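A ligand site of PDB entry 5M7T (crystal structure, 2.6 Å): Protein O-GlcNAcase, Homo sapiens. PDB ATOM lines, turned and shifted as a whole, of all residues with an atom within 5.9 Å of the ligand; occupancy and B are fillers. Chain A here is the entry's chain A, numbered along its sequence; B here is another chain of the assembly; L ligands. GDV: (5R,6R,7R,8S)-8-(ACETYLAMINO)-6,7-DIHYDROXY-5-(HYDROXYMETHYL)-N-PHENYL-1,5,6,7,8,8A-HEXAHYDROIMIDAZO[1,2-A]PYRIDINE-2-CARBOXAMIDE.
The side-chain carboxylate of Asp 285 is in hydrogen-bond range of the backbone NH of Tyr 69 (3.0 Å). OD1 of Asn 313 is in hydrogen-bond range of N of Gly 67 (3.0 Å). The side-chain hydroxyl (OH) of Tyr 69 is in hydrogen-bond range of the side-chain carboxylate (OD2) of Asp 175. ND2 of Asn 313 sits at hydrogen-bond distance from OD1 of Asn 280, 3.0 Å away. NE1 of Trp 278 sits at hydrogen-bond distance from OD1 of Asn 280 (3.0 Å). OD1 of Asn 313 lies within hydrogen-bond range of N of Phe 68 (3.3 Å). The backbone NH (N) of Ala 283 sits close to the backbone carbonyl oxygen (O) of Asn 313. The backbone carbonyl oxygen of Phe 68 lies within hydrogen-bond range of the backbone NH of Lys 98.
OD2 of Asp 285 is in hydrogen-bond range of O4 of the ligand (2.5 Å). An oxygen (O2) of the ligand sits at hydrogen-bond distance from the side-chain hydroxyl (OH) of Tyr 219 (2.7 Å). The backbone carbonyl oxygen (O) of Gly 67 lies within hydrogen-bond range of an oxygen (O3) of the ligand (2.7 Å). A nitrogen (N2) of the ligand lies within hydrogen-bond range of the side-chain carboxylate (OD1) of Asp 175 (2.8 Å). O1 of the ligand sits at hydrogen-bond distance from ND2 of Asn 280, 2.8 Å away. The side-chain amide nitrogen of Asn 313 lies within hydrogen-bond range of an oxygen (O4) of the ligand (2.9 Å). An oxygen (O3) of the ligand lies within hydrogen-bond range of the side-chain amino group (NZ) of Lys 98 (2.9 Å). OD2 of Asp 174 is in hydrogen-bond range of N4 of the ligand, 3.1 Å away. The indole nitrogen of Trp 278 lies within hydrogen-bond range of an oxygen (O1) of the ligand, at 3.3 Å.
CA of Phe 68 touches O4 of the ligand, at 3.6 Å. Tyr 69 touches the ligand. Phe 223 touches the ligand (CZ to O2, 3.5 Å). CG2 of Thr 250 touches C12 of the ligand, 3.8 Å away. CG1 of Val 254 touches C7 of the ligand, at 3.5 Å. CD2 of Tyr 286 touches O5 of the ligand, at 3.9 Å. Hydrophobic or aromatic side chains within 4 Å of the ligand: Phe 68, Tyr 69, Tyr 219, Phe 223, Val 254, Trp 278 and Tyr 286. Within 4 Å of the ligand: Gly 67, Phe 68, Tyr 69, Lys 98, Asp 174, Asp 175, Tyr 219, Phe 223, Thr 250, Val 254, Trp 278, Asn 280, Asp 285, Tyr 286 and Asn 313. The nearest printed residue that does not touch the ligand is Cys 215 (4.5 Å).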
ATOM      1  N   GLY A  67      12.366 -15.937  32.871  1.00  0.00           N
ATOM      2  CA  GLY A  67      11.177 -15.155  32.488  1.00  0.00           C
ATOM      3  C   GLY A  67       9.957 -15.973  32.089  1.00  0.00           C
ATOM      4  O   GLY A  67       9.076 -15.426  31.456  1.00  0.00           O
ATOM      5  N   PHE A  68       9.888 -17.226  32.505  1.00  0.00           N
ATOM      6  CA  PHE A  68       8.853 -18.162  31.975  1.00  0.00           C
ATOM      7  C   PHE A  68       7.684 -18.331  32.911  1.00  0.00           C
ATOM      8  O   PHE A  68       7.740 -17.895  34.062  1.00  0.00           O
ATOM      9  CB  PHE A  68       9.442 -19.525  31.667  1.00  0.00           C
ATOM     10  CG  PHE A  68      10.321 -20.064  32.769  1.00  0.00           C
ATOM     11  CD1 PHE A  68       9.765 -20.696  33.860  1.00  0.00           C
ATOM     12  CD2 PHE A  68      11.697 -19.983  32.683  1.00  0.00           C
ATOM     13  CE1 PHE A  68      10.551 -21.188  34.883  1.00  0.00           C
ATOM     14  CE2 PHE A  68      12.505 -20.516  33.688  1.00  0.00           C
ATOM     15  CZ  PHE A  68      11.926 -21.098  34.795  1.00  0.00           C
ATOM     16  N   TYR A  69       6.636 -18.998  32.432  1.00  0.00           N
ATOM     17  CA  TYR A  69       5.467 -19.340  33.241  1.00  0.00           C
ATOM     18  C   TYR A  69       5.661 -20.699  33.922  1.00  0.00           C
ATOM     19  O   TYR A  69       6.340 -21.561  33.443  1.00  0.00           O
ATOM     20  CB  TYR A  69       4.178 -19.391  32.401  1.00  0.00           C
ATOM     21  CG  TYR A  69       3.624 -18.050  31.905  1.00  0.00           C
ATOM     22  CD1 TYR A  69       4.026 -17.533  30.680  1.00  0.00           C
ATOM     23  CD2 TYR A  69       2.694 -17.337  32.622  1.00  0.00           C
ATOM     24  CE1 TYR A  69       3.525 -16.333  30.204  1.00  0.00           C
ATOM     25  CE2 TYR A  69       2.212 -16.128  32.170  1.00  0.00           C
ATOM     26  CZ  TYR A  69       2.627 -15.628  30.946  1.00  0.00           C
ATOM     27  OH  TYR A  69       2.159 -14.437  30.439  1.00  0.00           O
ATOM     28  N   LYS A  98       7.327 -15.406  35.804  1.00  0.00           N
ATOM     29  CA  LYS A  98       5.948 -14.940  35.640  1.00  0.00           C
ATOM     30  C   LYS A  98       5.070 -15.278  36.806  1.00  0.00           C
ATOM     31  O   LYS A  98       4.231 -14.502  37.146  1.00  0.00           O
ATOM     32  CB  LYS A  98       5.301 -15.520  34.363  1.00  0.00           C
ATOM     33  CG  LYS A  98       5.730 -14.806  33.096  1.00  0.00           C
ATOM     34  CD  LYS A  98       4.851 -13.599  32.794  1.00  0.00           C
ATOM     35  CE  LYS A  98       5.102 -12.929  31.469  1.00  0.00           C
ATOM     36  NZ  LYS A  98       6.553 -12.585  31.405  1.00  0.00           N
ATOM     37  N   ASP A 174       4.994  -6.884  28.791  1.00  0.00           N
ATOM     38  CA  ASP A 174       4.627  -8.003  27.948  1.00  0.00           C
ATOM     39  C   ASP A 174       3.366  -8.678  28.498  1.00  0.00           C
ATOM     40  O   ASP A 174       3.106  -8.647  29.675  1.00  0.00           O
ATOM     41  CB  ASP A 174       5.770  -9.017  27.897  1.00  0.00           C
ATOM     42  CG  ASP A 174       6.095  -9.636  29.269  1.00  0.00           C
ATOM     43  OD1 ASP A 174       6.478  -8.889  30.220  1.00  0.00           O
ATOM     44  OD2 ASP A 174       5.956 -10.872  29.375  1.00  0.00           O
ATOM     45  N   ASP A 175       2.585  -9.247  27.604  1.00  0.00           N
ATOM     46  CA  ASP A 175       1.444 -10.136  27.930  1.00  0.00           C
ATOM     47  C   ASP A 175       0.304  -9.467  28.678  1.00  0.00           C
ATOM     48  O   ASP A 175      -0.328 -10.080  29.528  1.00  0.00           O
ATOM     49  CB  ASP A 175       1.938 -11.374  28.703  1.00  0.00           C
ATOM     50  CG  ASP A 175       2.810 -12.304  27.858  1.00  0.00           C
ATOM     51  OD1 ASP A 175       3.401 -11.871  26.832  1.00  0.00           O
ATOM     52  OD2 ASP A 175       2.869 -13.515  28.228  1.00  0.00           O
ATOM     53  N   CYS A 215      10.518  -3.770  28.838  1.00  0.00           N
ATOM     54  CA  CYS A 215       9.936  -4.667  27.845  1.00  0.00           C
ATOM     55  C   CYS A 215       8.591  -4.142  27.347  1.00  0.00           C
ATOM     56  O   CYS A 215       7.632  -4.103  28.130  1.00  0.00           O
ATOM     57  CB  CYS A 215       9.727  -6.092  28.357  1.00  0.00           C
ATOM     58  SG  CYS A 215       8.984  -7.201  27.117  1.00  0.00           S
ATOM     59  N   TYR A 219       6.383  -6.395  21.691  1.00  0.00           N
ATOM     60  CA  TYR A 219       7.775  -6.805  21.911  1.00  0.00           C
ATOM     61  C   TYR A 219       8.392  -7.606  20.747  1.00  0.00           C
ATOM     62  O   TYR A 219       9.525  -8.089  20.859  1.00  0.00           O
ATOM     63  CB  TYR A 219       7.911  -7.560  23.244  1.00  0.00           C
ATOM     64  CG  TYR A 219       7.082  -8.802  23.363  1.00  0.00           C
ATOM     65  CD1 TYR A 219       7.457  -9.976  22.726  1.00  0.00           C
ATOM     66  CD2 TYR A 219       5.908  -8.812  24.103  1.00  0.00           C
ATOM     67  CE1 TYR A 219       6.687 -11.127  22.810  1.00  0.00           C
ATOM     68  CE2 TYR A 219       5.125  -9.972  24.205  1.00  0.00           C
ATOM     69  CZ  TYR A 219       5.520 -11.114  23.552  1.00  0.00           C
ATOM     70  OH  TYR A 219       4.769 -12.262  23.628  1.00  0.00           O
ATOM     71  N   PHE A 223       3.547  -8.613  16.715  1.00  0.00           N
ATOM     72  CA  PHE A 223       2.672  -7.906  17.656  1.00  0.00           C
ATOM     73  C   PHE A 223       2.593  -6.404  17.354  1.00  0.00           C
ATOM     74  O   PHE A 223       1.759  -5.741  17.910  1.00  0.00           O
ATOM     75  CB  PHE A 223       3.148  -8.089  19.095  1.00  0.00           C
ATOM     76  CG  PHE A 223       2.745  -9.398  19.741  1.00  0.00           C
ATOM     77  CD1 PHE A 223       2.602 -10.580  19.002  1.00  0.00           C
ATOM     78  CD2 PHE A 223       2.591  -9.471  21.117  1.00  0.00           C
ATOM     79  CE1 PHE A 223       2.268 -11.773  19.624  1.00  0.00           C
ATOM     80  CE2 PHE A 223       2.246 -10.656  21.741  1.00  0.00           C
ATOM     81  CZ  PHE A 223       2.081 -11.816  20.982  1.00  0.00           C
ATOM     82  N   THR A 250      11.924  -9.625  21.160  1.00  0.00           N
ATOM     83  CA  THR A 250      12.091 -11.073  20.934  1.00  0.00           C
ATOM     84  C   THR A 250      12.319 -11.487  19.492  1.00  0.00           C
ATOM     85  O   THR A 250      12.476 -12.670  19.240  1.00  0.00           O
ATOM     86  CB  THR A 250      10.928 -11.926  21.467  1.00  0.00           C
ATOM     87  OG1 THR A 250       9.802 -11.834  20.575  1.00  0.00           O
ATOM     88  CG2 THR A 250      10.525 -11.513  22.850  1.00  0.00           C
ATOM     89  N   VAL A 254       7.313 -14.088  18.542  1.00  0.00           N
ATOM     90  CA  VAL A 254       7.478 -14.456  19.944  1.00  0.00           C
ATOM     91  C   VAL A 254       8.578 -15.520  20.119  1.00  0.00           C
ATOM     92  O   VAL A 254       9.533 -15.327  20.859  1.00  0.00           O
ATOM     93  CB  VAL A 254       6.140 -14.998  20.517  1.00  0.00           C
ATOM     94  CG1 VAL A 254       6.321 -15.473  21.943  1.00  0.00           C
ATOM     95  CG2 VAL A 254       5.047 -13.957  20.433  1.00  0.00           C
ATOM     96  N   VAL A 255       8.430 -16.643  19.420  1.00  0.00           N
ATOM     97  CA  VAL A 255       9.513 -17.626  19.282  1.00  0.00           C
ATOM     98  C   VAL A 255      10.116 -17.538  17.866  1.00  0.00           C
ATOM     99  O   VAL A 255       9.703 -18.222  16.951  1.00  0.00           O
ATOM    100  CB  VAL A 255       9.033 -19.042  19.579  1.00  0.00           C
ATOM    101  CG1 VAL A 255      10.180 -20.020  19.495  1.00  0.00           C
ATOM    102  CG2 VAL A 255       8.405 -19.071  20.955  1.00  0.00           C
ATOM    103  N   TRP A 278      15.301 -10.569  24.219  1.00  0.00           N
ATOM    104  CA  TRP A 278      14.713 -11.584  25.100  1.00  0.00           C
ATOM    105  C   TRP A 278      14.485 -12.709  24.112  1.00  0.00           C
ATOM    106  O   TRP A 278      13.603 -12.625  23.257  1.00  0.00           O
ATOM    107  CB  TRP A 278      13.420 -11.070  25.725  1.00  0.00           C
ATOM    108  CG  TRP A 278      12.590 -12.025  26.509  1.00  0.00           C
ATOM    109  CD1 TRP A 278      12.086 -13.210  26.094  1.00  0.00           C
ATOM    110  CD2 TRP A 278      12.057 -11.804  27.815  1.00  0.00           C
ATOM    111  NE1 TRP A 278      11.298 -13.762  27.069  1.00  0.00           N
ATOM    112  CE2 TRP A 278      11.270 -12.933  28.140  1.00  0.00           C
ATOM    113  CE3 TRP A 278      12.158 -10.762  28.750  1.00  0.00           C
ATOM    114  CZ2 TRP A 278      10.599 -13.052  29.370  1.00  0.00           C
ATOM    115  CZ3 TRP A 278      11.506 -10.884  29.942  1.00  0.00           C
ATOM    116  CH2 TRP A 278      10.721 -12.017  30.244  1.00  0.00           C
ATOM    117  N   ASN A 280      13.372 -16.357  23.180  1.00  0.00           N
ATOM    118  CA  ASN A 280      12.503 -17.487  23.544  1.00  0.00           C
ATOM    119  C   ASN A 280      12.789 -18.754  22.756  1.00  0.00           C
ATOM    120  O   ASN A 280      12.008 -19.704  22.810  1.00  0.00           O
ATOM    121  CB  ASN A 280      11.044 -17.123  23.327  1.00  0.00           C
ATOM    122  CG  ASN A 280      10.539 -16.100  24.314  1.00  0.00           C
ATOM    123  OD1 ASN A 280      10.688 -16.261  25.511  1.00  0.00           O
ATOM    124  ND2 ASN A 280       9.913 -15.071  23.809  1.00  0.00           N
ATOM    125  N   ALA A 283      12.595 -21.730  25.126  1.00  0.00           N
ATOM    126  CA  ALA A 283      11.494 -21.715  26.064  1.00  0.00           C
ATOM    127  C   ALA A 283      10.523 -22.872  25.771  1.00  0.00           C
ATOM    128  O   ALA A 283      10.224 -23.157  24.618  1.00  0.00           O
ATOM    129  CB  ALA A 283      10.768 -20.360  25.963  1.00  0.00           C
ATOM    130  N   ASP A 285       7.569 -23.467  28.213  1.00  0.00           N
ATOM    131  CA  ASP A 285       6.357 -23.297  29.014  1.00  0.00           C
ATOM    132  C   ASP A 285       5.081 -23.418  28.234  1.00  0.00           C
ATOM    133  O   ASP A 285       4.051 -23.719  28.807  1.00  0.00           O
ATOM    134  CB  ASP A 285       6.349 -21.954  29.794  1.00  0.00           C
ATOM    135  CG  ASP A 285       6.570 -20.715  28.903  1.00  0.00           C
ATOM    136  OD1 ASP A 285       6.579 -20.890  27.668  1.00  0.00           O
ATOM    137  OD2 ASP A 285       6.769 -19.598  29.454  1.00  0.00           O
ATOM    138  N   TYR A 286       5.133 -23.208  26.932  1.00  0.00           N
ATOM    139  CA  TYR A 286       3.931 -23.198  26.089  1.00  0.00           C
ATOM    140  C   TYR A 286       3.448 -24.570  25.597  1.00  0.00           C
ATOM    141  O   TYR A 286       2.379 -24.625  25.011  1.00  0.00           O
ATOM    142  CB  TYR A 286       4.060 -22.213  24.917  1.00  0.00           C
ATOM    143  CG  TYR A 286       5.177 -22.521  24.011  1.00  0.00           C
ATOM    144  CD1 TYR A 286       5.050 -23.516  23.028  1.00  0.00           C
ATOM    145  CD2 TYR A 286       6.384 -21.884  24.136  1.00  0.00           C
ATOM    146  CE1 TYR A 286       6.090 -23.838  22.197  1.00  0.00           C
ATOM    147  CE2 TYR A 286       7.444 -22.225  23.292  1.00  0.00           C
ATOM    148  CZ  TYR A 286       7.265 -23.181  22.306  1.00  0.00           C
ATOM    149  OH  TYR A 286       8.324 -23.533  21.510  1.00  0.00           O
ATOM    150  N   ASN A 313      15.575 -16.889  27.540  1.00  0.00           N
ATOM    151  CA  ASN A 313      14.502 -17.415  28.410  1.00  0.00           C
ATOM    152  C   ASN A 313      14.313 -18.943  28.156  1.00  0.00           C
ATOM    153  O   ASN A 313      13.517 -19.341  27.295  1.00  0.00           O
ATOM    154  CB  ASN A 313      13.189 -16.666  28.058  1.00  0.00           C
ATOM    155  CG  ASN A 313      12.031 -17.003  28.982  1.00  0.00           C
ATOM    156  OD1 ASN A 313      12.219 -17.168  30.166  1.00  0.00           O
ATOM    157  ND2 ASN A 313      10.797 -17.079  28.437  1.00  0.00           N
ATOM    158  N   TRP B 645      -2.469 -25.161  32.496  1.00  0.00           N
ATOM    159  CA  TRP B 645      -2.073 -24.286  31.404  1.00  0.00           C
ATOM    160  C   TRP B 645      -2.412 -24.949  30.075  1.00  0.00           C
ATOM    161  O   TRP B 645      -2.745 -24.301  29.081  1.00  0.00           O
ATOM    162  CB  TRP B 645      -0.588 -23.898  31.469  1.00  0.00           C
ATOM    163  CG  TRP B 645      -0.123 -23.065  30.288  1.00  0.00           C
ATOM    164  CD1 TRP B 645       0.159 -23.516  29.023  1.00  0.00           C
ATOM    165  CD2 TRP B 645       0.093 -21.649  30.258  1.00  0.00           C
ATOM    166  NE1 TRP B 645       0.530 -22.476  28.211  1.00  0.00           N
ATOM    167  CE2 TRP B 645       0.502 -21.314  28.950  1.00  0.00           C
ATOM    168  CE3 TRP B 645      -0.039 -20.640  31.195  1.00  0.00           C
ATOM    169  CZ2 TRP B 645       0.817 -20.004  28.575  1.00  0.00           C
ATOM    170  CZ3 TRP B 645       0.283 -19.319  30.816  1.00  0.00           C
ATOM    171  CH2 TRP B 645       0.716 -19.028  29.522  1.00  0.00           C
ATOM    172  N   MET B 653      -7.687 -22.070  21.963  1.00  0.00           N
ATOM    173  CA  MET B 653      -7.548 -22.316  20.527  1.00  0.00           C
ATOM    174  C   MET B 653      -8.830 -22.855  19.919  1.00  0.00           C
ATOM    175  O   MET B 653      -9.247 -22.397  18.854  1.00  0.00           O
ATOM    176  CB  MET B 653      -6.377 -23.252  20.247  1.00  0.00           C
ATOM    177  CG  MET B 653      -5.058 -22.473  20.218  1.00  0.00           C
ATOM    178  SD  MET B 653      -4.763 -21.394  18.787  1.00  0.00           S
ATOM    179  CE  MET B 653      -3.894 -20.015  19.547  1.00  0.00           C
ATOM    180  N   TRP B 679       3.347 -24.800  16.731  1.00  0.00           N
ATOM    181  CA  TRP B 679       1.984 -25.416  16.687  1.00  0.00           C
ATOM    182  C   TRP B 679       1.842 -26.525  15.621  1.00  0.00           C
ATOM    183  O   TRP B 679       1.191 -27.531  15.875  1.00  0.00           O
ATOM    184  CB  TRP B 679       0.872 -24.362  16.476  1.00  0.00           C
ATOM    185  CG  TRP B 679       0.202 -23.998  17.769  1.00  0.00           C
ATOM    186  CD1 TRP B 679       0.502 -22.931  18.583  1.00  0.00           C
ATOM    187  CD2 TRP B 679      -0.863 -24.712  18.414  1.00  0.00           C
ATOM    188  NE1 TRP B 679      -0.323 -22.933  19.692  1.00  0.00           N
ATOM    189  CE2 TRP B 679      -1.167 -24.007  19.616  1.00  0.00           C
ATOM    190  CE3 TRP B 679      -1.607 -25.862  18.095  1.00  0.00           C
ATOM    191  CZ2 TRP B 679      -2.166 -24.435  20.521  1.00  0.00           C
ATOM    192  CZ3 TRP B 679      -2.630 -26.286  18.995  1.00  0.00           C
ATOM    193  CH2 TRP B 679      -2.904 -25.546  20.177  1.00  0.00           C
HETATM  194  O1  GDV L   1       8.282 -13.843  25.722  1.00  0.00           O
HETATM  195  C10 GDV L   1       7.910 -12.870  26.337  1.00  0.00           C
HETATM  196  C12 GDV L   1       8.588 -11.542  26.149  1.00  0.00           C
HETATM  197  N4  GDV L   1       6.931 -12.932  27.221  1.00  0.00           N
HETATM  198  C2  GDV L   1       6.260 -14.156  27.608  1.00  0.00           C
HETATM  199  C3  GDV L   1       7.197 -15.186  28.323  1.00  0.00           C
HETATM  200  O3  GDV L   1       7.075 -14.921  29.726  1.00  0.00           O
HETATM  201  C4  GDV L   1       6.934 -16.686  27.977  1.00  0.00           C
HETATM  202  O4  GDV L   1       7.922 -17.563  28.554  1.00  0.00           O
HETATM  203  C5  GDV L   1       6.895 -16.838  26.434  1.00  0.00           C
HETATM  204  C6  GDV L   1       6.752 -18.252  25.902  1.00  0.00           C
HETATM  205  O5  GDV L   1       5.506 -18.774  26.360  1.00  0.00           O
HETATM  206  C1  GDV L   1       5.511 -14.793  26.491  1.00  0.00           C
HETATM  207  N1  GDV L   1       5.755 -16.006  25.976  1.00  0.00           N
HETATM  208  C7  GDV L   1       4.829 -16.251  25.042  1.00  0.00           C
HETATM  209  C8  GDV L   1       3.982 -15.166  24.992  1.00  0.00           C
HETATM  210  N2  GDV L   1       4.427 -14.297  25.900  1.00  0.00           N
HETATM  211  C9  GDV L   1       2.813 -14.965  24.118  1.00  0.00           C
HETATM  212  O2  GDV L   1       2.633 -13.837  23.737  1.00  0.00           O
HETATM  213  N3  GDV L   1       2.081 -16.037  23.806  1.00  0.00           N
HETATM  214  C11 GDV L   1       1.090 -16.152  22.869  1.00  0.00           C
HETATM  215  C17 GDV L   1       0.567 -17.446  22.666  1.00  0.00           C
HETATM  216  C16 GDV L   1      -0.441 -17.671  21.722  1.00  0.00           C
HETATM  217  C15 GDV L   1      -0.933 -16.607  20.963  1.00  0.00           C
HETATM  218  C14 GDV L   1      -0.414 -15.327  21.150  1.00  0.00           C
HETATM  219  C13 GDV L   1       0.591 -15.105  22.085  1.00  0.00           C
